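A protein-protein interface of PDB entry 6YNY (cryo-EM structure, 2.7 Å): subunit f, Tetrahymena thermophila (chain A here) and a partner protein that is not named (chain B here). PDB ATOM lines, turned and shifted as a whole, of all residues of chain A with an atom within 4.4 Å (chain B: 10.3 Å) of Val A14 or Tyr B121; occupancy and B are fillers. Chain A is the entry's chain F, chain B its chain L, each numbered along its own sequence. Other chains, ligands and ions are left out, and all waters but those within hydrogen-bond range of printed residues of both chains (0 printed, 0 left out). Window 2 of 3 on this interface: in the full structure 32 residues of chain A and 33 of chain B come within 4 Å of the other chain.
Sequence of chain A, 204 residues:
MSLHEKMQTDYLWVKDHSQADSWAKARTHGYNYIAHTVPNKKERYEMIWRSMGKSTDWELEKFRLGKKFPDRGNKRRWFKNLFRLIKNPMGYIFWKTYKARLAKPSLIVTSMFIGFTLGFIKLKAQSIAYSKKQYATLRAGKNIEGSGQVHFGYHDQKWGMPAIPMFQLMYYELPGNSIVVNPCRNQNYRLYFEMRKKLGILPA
A ring nitrogen (ND1) of His A17 is in hydrogen-bond range of the side-chain amide nitrogen of Asn B119 (3.4 Å).
O of Lys A15 lies close to NE2 of His A17, 3.4 Å away.
The backbone NH (N) of Tyr B121 lies within hydrogen-bond range of the side-chain amide oxygen (OD1) of Asn B119 (2.7 Å).
Among the printed residues, merely in contact across the chains: Val A14 with Phe B120, Val A14 with Tyr B121, His A17 with Tyr B121, Lys A80 with Tyr B121, Phe A83 with Phe B120, Phe A83 with Tyr B121 and Phe A83 with Val B124.
Trp A13 touches none of the printed residues of chain B.
Of chain B, only Phe B120 (3.7 Å) and Tyr B121 (3.97 Å) come within 4 Å of Val A14.
Of the printed residues of chain B, His A17 touches Asn B119 and Tyr B121.
Lys A80 touches one residue of chain B.
Printed residues of chain A within 4 Å of Phe B120: Val A14 and Phe A83.
Printed residues of chain A within 4 Å of Tyr B121: Val A14 (3.97 Å), His A17 (3.6 Å), Lys A80 (3.6 Å) and Phe A83 (3.98 Å).
Arg B123 touches none of the printed residues of chain A.
Of the printed residues of chain A, Val B124 touches Phe A83 (3.7 Å).
Met B127 touches none of the printed residues of chain A.
The nearest residue of chain B that does not touch Val A14 is Asn B119 (6.3 Å).
Of the 6 printed residues of chain A, 4 touch a printed residue of chain B.
Hydrophobic or aromatic side chains of chain A within 4 Å of the printed part of chain B: Val A14, His A17 and Phe A83.
Of the 13 printed residues of chain B, 4 touch a printed residue of chain A.
Printed residues of chain B that touch a printed residue of chain A: Asn B119, Phe B120, Tyr B121 and Val B124.
Hydrophobic or aromatic side chains of chain B that line the printed part of chain A: Phe B120, Tyr B121 and Val B124.
Among the printed residues, 8 pairs touch across the chains.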
ATOM      1  N   TRP A  13      28.642 -17.645  10.327  1.00  0.00           N
ATOM      2  CA  TRP A  13      27.970 -18.203   9.165  1.00  0.00           C
ATOM      3  C   TRP A  13      26.679 -18.889   9.585  1.00  0.00           C
ATOM      4  O   TRP A  13      26.448 -19.165  10.765  1.00  0.00           O
ATOM      5  CB  TRP A  13      28.898 -19.171   8.424  1.00  0.00           C
ATOM      6  CG  TRP A  13      28.435 -19.535   7.059  1.00  0.00           C
ATOM      7  CD1 TRP A  13      28.268 -20.787   6.564  1.00  0.00           C
ATOM      8  CD2 TRP A  13      28.070 -18.636   6.009  1.00  0.00           C
ATOM      9  NE1 TRP A  13      27.824 -20.731   5.270  1.00  0.00           N
ATOM     10  CE2 TRP A  13      27.693 -19.419   4.905  1.00  0.00           C
ATOM     11  CE3 TRP A  13      28.024 -17.245   5.895  1.00  0.00           C
ATOM     12  CZ2 TRP A  13      27.278 -18.859   3.705  1.00  0.00           C
ATOM     13  CZ3 TRP A  13      27.614 -16.695   4.706  1.00  0.00           C
ATOM     14  CH2 TRP A  13      27.244 -17.498   3.626  1.00  0.00           C
ATOM     15  N   VAL A  14      25.831 -19.161   8.593  1.00  0.00           N
ATOM     16  CA  VAL A  14      24.531 -19.785   8.799  1.00  0.00           C
ATOM     17  C   VAL A  14      24.634 -21.251   8.432  1.00  0.00           C
ATOM     18  O   VAL A  14      25.394 -21.642   7.540  1.00  0.00           O
ATOM     19  CB  VAL A  14      23.424 -19.107   7.965  1.00  0.00           C
ATOM     20  CG1 VAL A  14      22.091 -19.751   8.246  1.00  0.00           C
ATOM     21  CG2 VAL A  14      23.350 -17.665   8.269  1.00  0.00           C
ATOM     22  N   LYS A  15      23.857 -22.073   9.124  1.00  0.00           N
ATOM     23  CA  LYS A  15      23.664 -23.460   8.748  1.00  0.00           C
ATOM     24  C   LYS A  15      22.284 -23.640   8.136  1.00  0.00           C
ATOM     25  O   LYS A  15      21.396 -22.797   8.285  1.00  0.00           O
ATOM     26  CB  LYS A  15      23.819 -24.379   9.958  1.00  0.00           C
ATOM     27  CG  LYS A  15      25.258 -24.637  10.360  1.00  0.00           C
ATOM     28  CD  LYS A  15      25.381 -25.916  11.160  1.00  0.00           C
ATOM     29  CE  LYS A  15      26.822 -26.363  11.257  1.00  0.00           C
ATOM     30  NZ  LYS A  15      26.936 -27.754  11.784  1.00  0.00           N
ATOM     31  N   HIS A  17      18.809 -25.166   8.198  1.00  0.00           N
ATOM     32  CA  HIS A  17      17.950 -25.650   9.266  1.00  0.00           C
ATOM     33  C   HIS A  17      16.993 -26.734   8.802  1.00  0.00           C
ATOM     34  O   HIS A  17      16.509 -27.511   9.630  1.00  0.00           O
ATOM     35  CB  HIS A  17      17.152 -24.491   9.853  1.00  0.00           C
ATOM     36  CG  HIS A  17      18.001 -23.349  10.310  1.00  0.00           C
ATOM     37  ND1 HIS A  17      17.514 -22.069  10.451  1.00  0.00           N
ATOM     38  CD2 HIS A  17      19.308 -23.294  10.658  1.00  0.00           C
ATOM     39  CE1 HIS A  17      18.484 -21.275  10.864  1.00  0.00           C
ATOM     40  NE2 HIS A  17      19.583 -21.993  10.997  1.00  0.00           N
ATOM     41  N   LYS A  80      16.634 -17.196   0.621  1.00  0.00           N
ATOM     42  CA  LYS A  80      17.813 -17.333   1.466  1.00  0.00           C
ATOM     43  C   LYS A  80      19.017 -16.604   0.884  1.00  0.00           C
ATOM     44  O   LYS A  80      19.829 -16.046   1.630  1.00  0.00           O
ATOM     45  CB  LYS A  80      18.122 -18.811   1.666  1.00  0.00           C
ATOM     46  CG  LYS A  80      17.135 -19.513   2.560  1.00  0.00           C
ATOM     47  CD  LYS A  80      17.349 -21.002   2.562  1.00  0.00           C
ATOM     48  CE  LYS A  80      16.377 -21.686   3.487  1.00  0.00           C
ATOM     49  NZ  LYS A  80      16.617 -23.139   3.562  1.00  0.00           N
ATOM     50  N   PHE A  83      18.549 -12.826   1.576  1.00  0.00           N
ATOM     51  CA  PHE A  83      18.839 -12.417   2.944  1.00  0.00           C
ATOM     52  C   PHE A  83      20.335 -12.365   3.215  1.00  0.00           C
ATOM     53  O   PHE A  83      20.784 -11.567   4.045  1.00  0.00           O
ATOM     54  CB  PHE A  83      18.152 -13.363   3.924  1.00  0.00           C
ATOM     55  CG  PHE A  83      16.667 -13.453   3.742  1.00  0.00           C
ATOM     56  CD1 PHE A  83      15.937 -12.365   3.307  1.00  0.00           C
ATOM     57  CD2 PHE A  83      15.999 -14.631   4.008  1.00  0.00           C
ATOM     58  CE1 PHE A  83      14.575 -12.453   3.143  1.00  0.00           C
ATOM     59  CE2 PHE A  83      14.639 -14.717   3.844  1.00  0.00           C
ATOM     60  CZ  PHE A  83      13.928 -13.628   3.410  1.00  0.00           C
ATOM     61  N   LEU B 117      18.286 -13.151  19.501  1.00  0.00           N
ATOM     62  CA  LEU B 117      17.590 -14.188  18.757  1.00  0.00           C
ATOM     63  C   LEU B 117      18.593 -15.124  18.103  1.00  0.00           C
ATOM     64  O   LEU B 117      19.532 -14.681  17.436  1.00  0.00           O
ATOM     65  CB  LEU B 117      16.681 -13.565  17.705  1.00  0.00           C
ATOM     66  CG  LEU B 117      15.411 -12.896  18.216  1.00  0.00           C
ATOM     67  CD1 LEU B 117      14.679 -12.235  17.081  1.00  0.00           C
ATOM     68  CD2 LEU B 117      14.523 -13.911  18.880  1.00  0.00           C
ATOM     69  N   ARG B 118      18.391 -16.424  18.294  1.00  0.00           N
ATOM     70  CA  ARG B 118      19.368 -17.402  17.839  1.00  0.00           C
ATOM     71  C   ARG B 118      19.271 -17.626  16.336  1.00  0.00           C
ATOM     72  O   ARG B 118      20.278 -17.554  15.625  1.00  0.00           O
ATOM     73  CB  ARG B 118      19.168 -18.709  18.601  1.00  0.00           C
ATOM     74  CG  ARG B 118      20.051 -19.838  18.149  1.00  0.00           C
ATOM     75  CD  ARG B 118      20.903 -20.356  19.273  1.00  0.00           C
ATOM     76  NE  ARG B 118      21.655 -21.531  18.858  1.00  0.00           N
ATOM     77  CZ  ARG B 118      22.775 -21.488  18.148  1.00  0.00           C
ATOM     78  NH1 ARG B 118      23.284 -20.326  17.771  1.00  0.00           N
ATOM     79  NH2 ARG B 118      23.384 -22.612  17.811  1.00  0.00           N
ATOM     80  N   ASN B 119      18.073 -17.906  15.835  1.00  0.00           N
ATOM     81  CA  ASN B 119      17.904 -18.196  14.420  1.00  0.00           C
ATOM     82  C   ASN B 119      18.127 -16.941  13.589  1.00  0.00           C
ATOM     83  O   ASN B 119      17.581 -15.876  13.889  1.00  0.00           O
ATOM     84  CB  ASN B 119      16.513 -18.760  14.159  1.00  0.00           C
ATOM     85  CG  ASN B 119      16.369 -19.333  12.772  1.00  0.00           C
ATOM     86  OD1 ASN B 119      16.955 -18.837  11.814  1.00  0.00           O
ATOM     87  ND2 ASN B 119      15.584 -20.388  12.656  1.00  0.00           N
ATOM     88  N   PHE B 120      18.942 -17.069  12.543  1.00  0.00           N
ATOM     89  CA  PHE B 120      19.200 -15.940  11.661  1.00  0.00           C
ATOM     90  C   PHE B 120      17.950 -15.518  10.907  1.00  0.00           C
ATOM     91  O   PHE B 120      17.762 -14.326  10.642  1.00  0.00           O
ATOM     92  CB  PHE B 120      20.317 -16.294  10.684  1.00  0.00           C
ATOM     93  CG  PHE B 120      20.400 -15.383   9.501  1.00  0.00           C
ATOM     94  CD1 PHE B 120      20.790 -14.069   9.648  1.00  0.00           C
ATOM     95  CD2 PHE B 120      20.100 -15.842   8.238  1.00  0.00           C
ATOM     96  CE1 PHE B 120      20.867 -13.236   8.565  1.00  0.00           C
ATOM     97  CE2 PHE B 120      20.177 -15.012   7.154  1.00  0.00           C
ATOM     98  CZ  PHE B 120      20.563 -13.706   7.318  1.00  0.00           C
ATOM     99  N   TYR B 121      17.089 -16.469  10.555  1.00  0.00           N
ATOM    100  CA  TYR B 121      15.893 -16.163   9.787  1.00  0.00           C
ATOM    101  C   TYR B 121      14.771 -15.598  10.644  1.00  0.00           C
ATOM    102  O   TYR B 121      13.810 -15.051  10.095  1.00  0.00           O
ATOM    103  CB  TYR B 121      15.423 -17.416   9.049  1.00  0.00           C
ATOM    104  CG  TYR B 121      16.452 -17.943   8.086  1.00  0.00           C
ATOM    105  CD1 TYR B 121      17.225 -19.043   8.402  1.00  0.00           C
ATOM    106  CD2 TYR B 121      16.664 -17.327   6.866  1.00  0.00           C
ATOM    107  CE1 TYR B 121      18.169 -19.523   7.530  1.00  0.00           C
ATOM    108  CE2 TYR B 121      17.606 -17.797   5.989  1.00  0.00           C
ATOM    109  CZ  TYR B 121      18.358 -18.896   6.325  1.00  0.00           C
ATOM    110  OH  TYR B 121      19.303 -19.373   5.451  1.00  0.00           O
ATOM    111  N   ALA B 122      14.862 -15.721  11.966  1.00  0.00           N
ATOM    112  CA  ALA B 122      13.904 -15.060  12.840  1.00  0.00           C
ATOM    113  C   ALA B 122      14.191 -13.571  12.944  1.00  0.00           C
ATOM    114  O   ALA B 122      13.265 -12.759  13.033  1.00  0.00           O
ATOM    115  CB  ALA B 122      13.925 -15.700  14.223  1.00  0.00           C
ATOM    116  N   ARG B 123      15.471 -13.197  12.949  1.00  0.00           N
ATOM    117  CA  ARG B 123      15.830 -11.788  12.895  1.00  0.00           C
ATOM    118  C   ARG B 123      15.555 -11.200  11.519  1.00  0.00           C
ATOM    119  O   ARG B 123      15.330  -9.992  11.395  1.00  0.00           O
ATOM    120  CB  ARG B 123      17.296 -11.616  13.275  1.00  0.00           C
ATOM    121  CG  ARG B 123      17.658 -12.272  14.581  1.00  0.00           C
ATOM    122  CD  ARG B 123      19.018 -11.859  15.066  1.00  0.00           C
ATOM    123  NE  ARG B 123      20.062 -12.097  14.077  1.00  0.00           N
ATOM    124  CZ  ARG B 123      20.766 -13.214  13.974  1.00  0.00           C
ATOM    125  NH1 ARG B 123      20.553 -14.227  14.795  1.00  0.00           N
ATOM    126  NH2 ARG B 123      21.687 -13.318  13.038  1.00  0.00           N
ATOM    127  N   VAL B 124      15.575 -12.035  10.480  1.00  0.00           N
ATOM    128  CA  VAL B 124      15.128 -11.602   9.161  1.00  0.00           C
ATOM    129  C   VAL B 124      13.694 -11.099   9.230  1.00  0.00           C
ATOM    130  O   VAL B 124      13.332 -10.112   8.581  1.00  0.00           O
ATOM    131  CB  VAL B 124      15.283 -12.753   8.150  1.00  0.00           C
ATOM    132  CG1 VAL B 124      14.604 -12.423   6.849  1.00  0.00           C
ATOM    133  CG2 VAL B 124      16.741 -13.050   7.906  1.00  0.00           C
ATOM    134  N   PHE B 125      12.855 -11.771  10.021  1.00  0.00           N
ATOM    135  CA  PHE B 125      11.472 -11.341  10.181  1.00  0.00           C
ATOM    136  C   PHE B 125      11.384 -10.051  10.983  1.00  0.00           C
ATOM    137  O   PHE B 125      10.596  -9.159  10.654  1.00  0.00           O
ATOM    138  CB  PHE B 125      10.662 -12.447  10.855  1.00  0.00           C
ATOM    139  CG  PHE B 125       9.272 -12.036  11.233  1.00  0.00           C
ATOM    140  CD1 PHE B 125       8.230 -12.154  10.334  1.00  0.00           C
ATOM    141  CD2 PHE B 125       9.004 -11.532  12.494  1.00  0.00           C
ATOM    142  CE1 PHE B 125       6.954 -11.777  10.685  1.00  0.00           C
ATOM    143  CE2 PHE B 125       7.731 -11.154  12.846  1.00  0.00           C
ATOM    144  CZ  PHE B 125       6.705 -11.276  11.941  1.00  0.00           C
ATOM    145  N   VAL B 126      12.189  -9.934  12.038  1.00  0.00           N
ATOM    146  CA  VAL B 126      12.166  -8.733  12.865  1.00  0.00           C
ATOM    147  C   VAL B 126      12.585  -7.519  12.050  1.00  0.00           C
ATOM    148  O   VAL B 126      11.930  -6.472  12.079  1.00  0.00           O
ATOM    149  CB  VAL B 126      13.066  -8.920  14.096  1.00  0.00           C
ATOM    150  CG1 VAL B 126      13.233  -7.616  14.828  1.00  0.00           C
ATOM    151  CG2 VAL B 126      12.484  -9.964  15.011  1.00  0.00           C
ATOM    152  N   MET B 127      13.689  -7.638  11.314  1.00  0.00           N
ATOM    153  CA  MET B 127      14.142  -6.523  10.495  1.00  0.00           C
ATOM    154  C   MET B 127      13.169  -6.220   9.370  1.00  0.00           C
ATOM    155  O   MET B 127      13.067  -5.069   8.935  1.00  0.00           O
ATOM    156  CB  MET B 127      15.531  -6.821   9.943  1.00  0.00           C
ATOM    157  CG  MET B 127      16.617  -6.601  10.954  1.00  0.00           C
ATOM    158  SD  MET B 127      16.747  -4.869  11.401  1.00  0.00           S
ATOM    159  CE  MET B 127      17.671  -5.023  12.908  1.00  0.00           C
ATOM    160  N   TYR B 128      12.449  -7.231   8.888  1.00  0.00           N
ATOM    161  CA  TYR B 128      11.406  -6.981   7.904  1.00  0.00           C
ATOM    162  C   TYR B 128      10.275  -6.162   8.509  1.00  0.00           C
ATOM    163  O   TYR B 128       9.683  -5.314   7.832  1.00  0.00           O
ATOM    164  CB  TYR B 128      10.882  -8.304   7.358  1.00  0.00           C
ATOM    165  CG  TYR B 128       9.712  -8.151   6.426  1.00  0.00           C
ATOM    166  CD1 TYR B 128       9.845  -7.479   5.228  1.00  0.00           C
ATOM    167  CD2 TYR B 128       8.477  -8.683   6.743  1.00  0.00           C
ATOM    168  CE1 TYR B 128       8.783  -7.335   4.376  1.00  0.00           C
ATOM    169  CE2 TYR B 128       7.408  -8.545   5.894  1.00  0.00           C
ATOM    170  CZ  TYR B 128       7.567  -7.869   4.712  1.00  0.00           C
ATOM    171  OH  TYR B 128       6.502  -7.730   3.861  1.00  0.00           O
ATOM    172  N   ALA B 129       9.964  -6.399   9.782  1.00  0.00           N
ATOM    173  CA  ALA B 129       8.935  -5.614  10.451  1.00  0.00           C
ATOM    174  C   ALA B 129       9.427  -4.209  10.768  1.00  0.00           C
ATOM    175  O   ALA B 129       8.665  -3.241  10.672  1.00  0.00           O
ATOM    176  CB  ALA B 129       8.489  -6.320  11.726  1.00  0.00           C
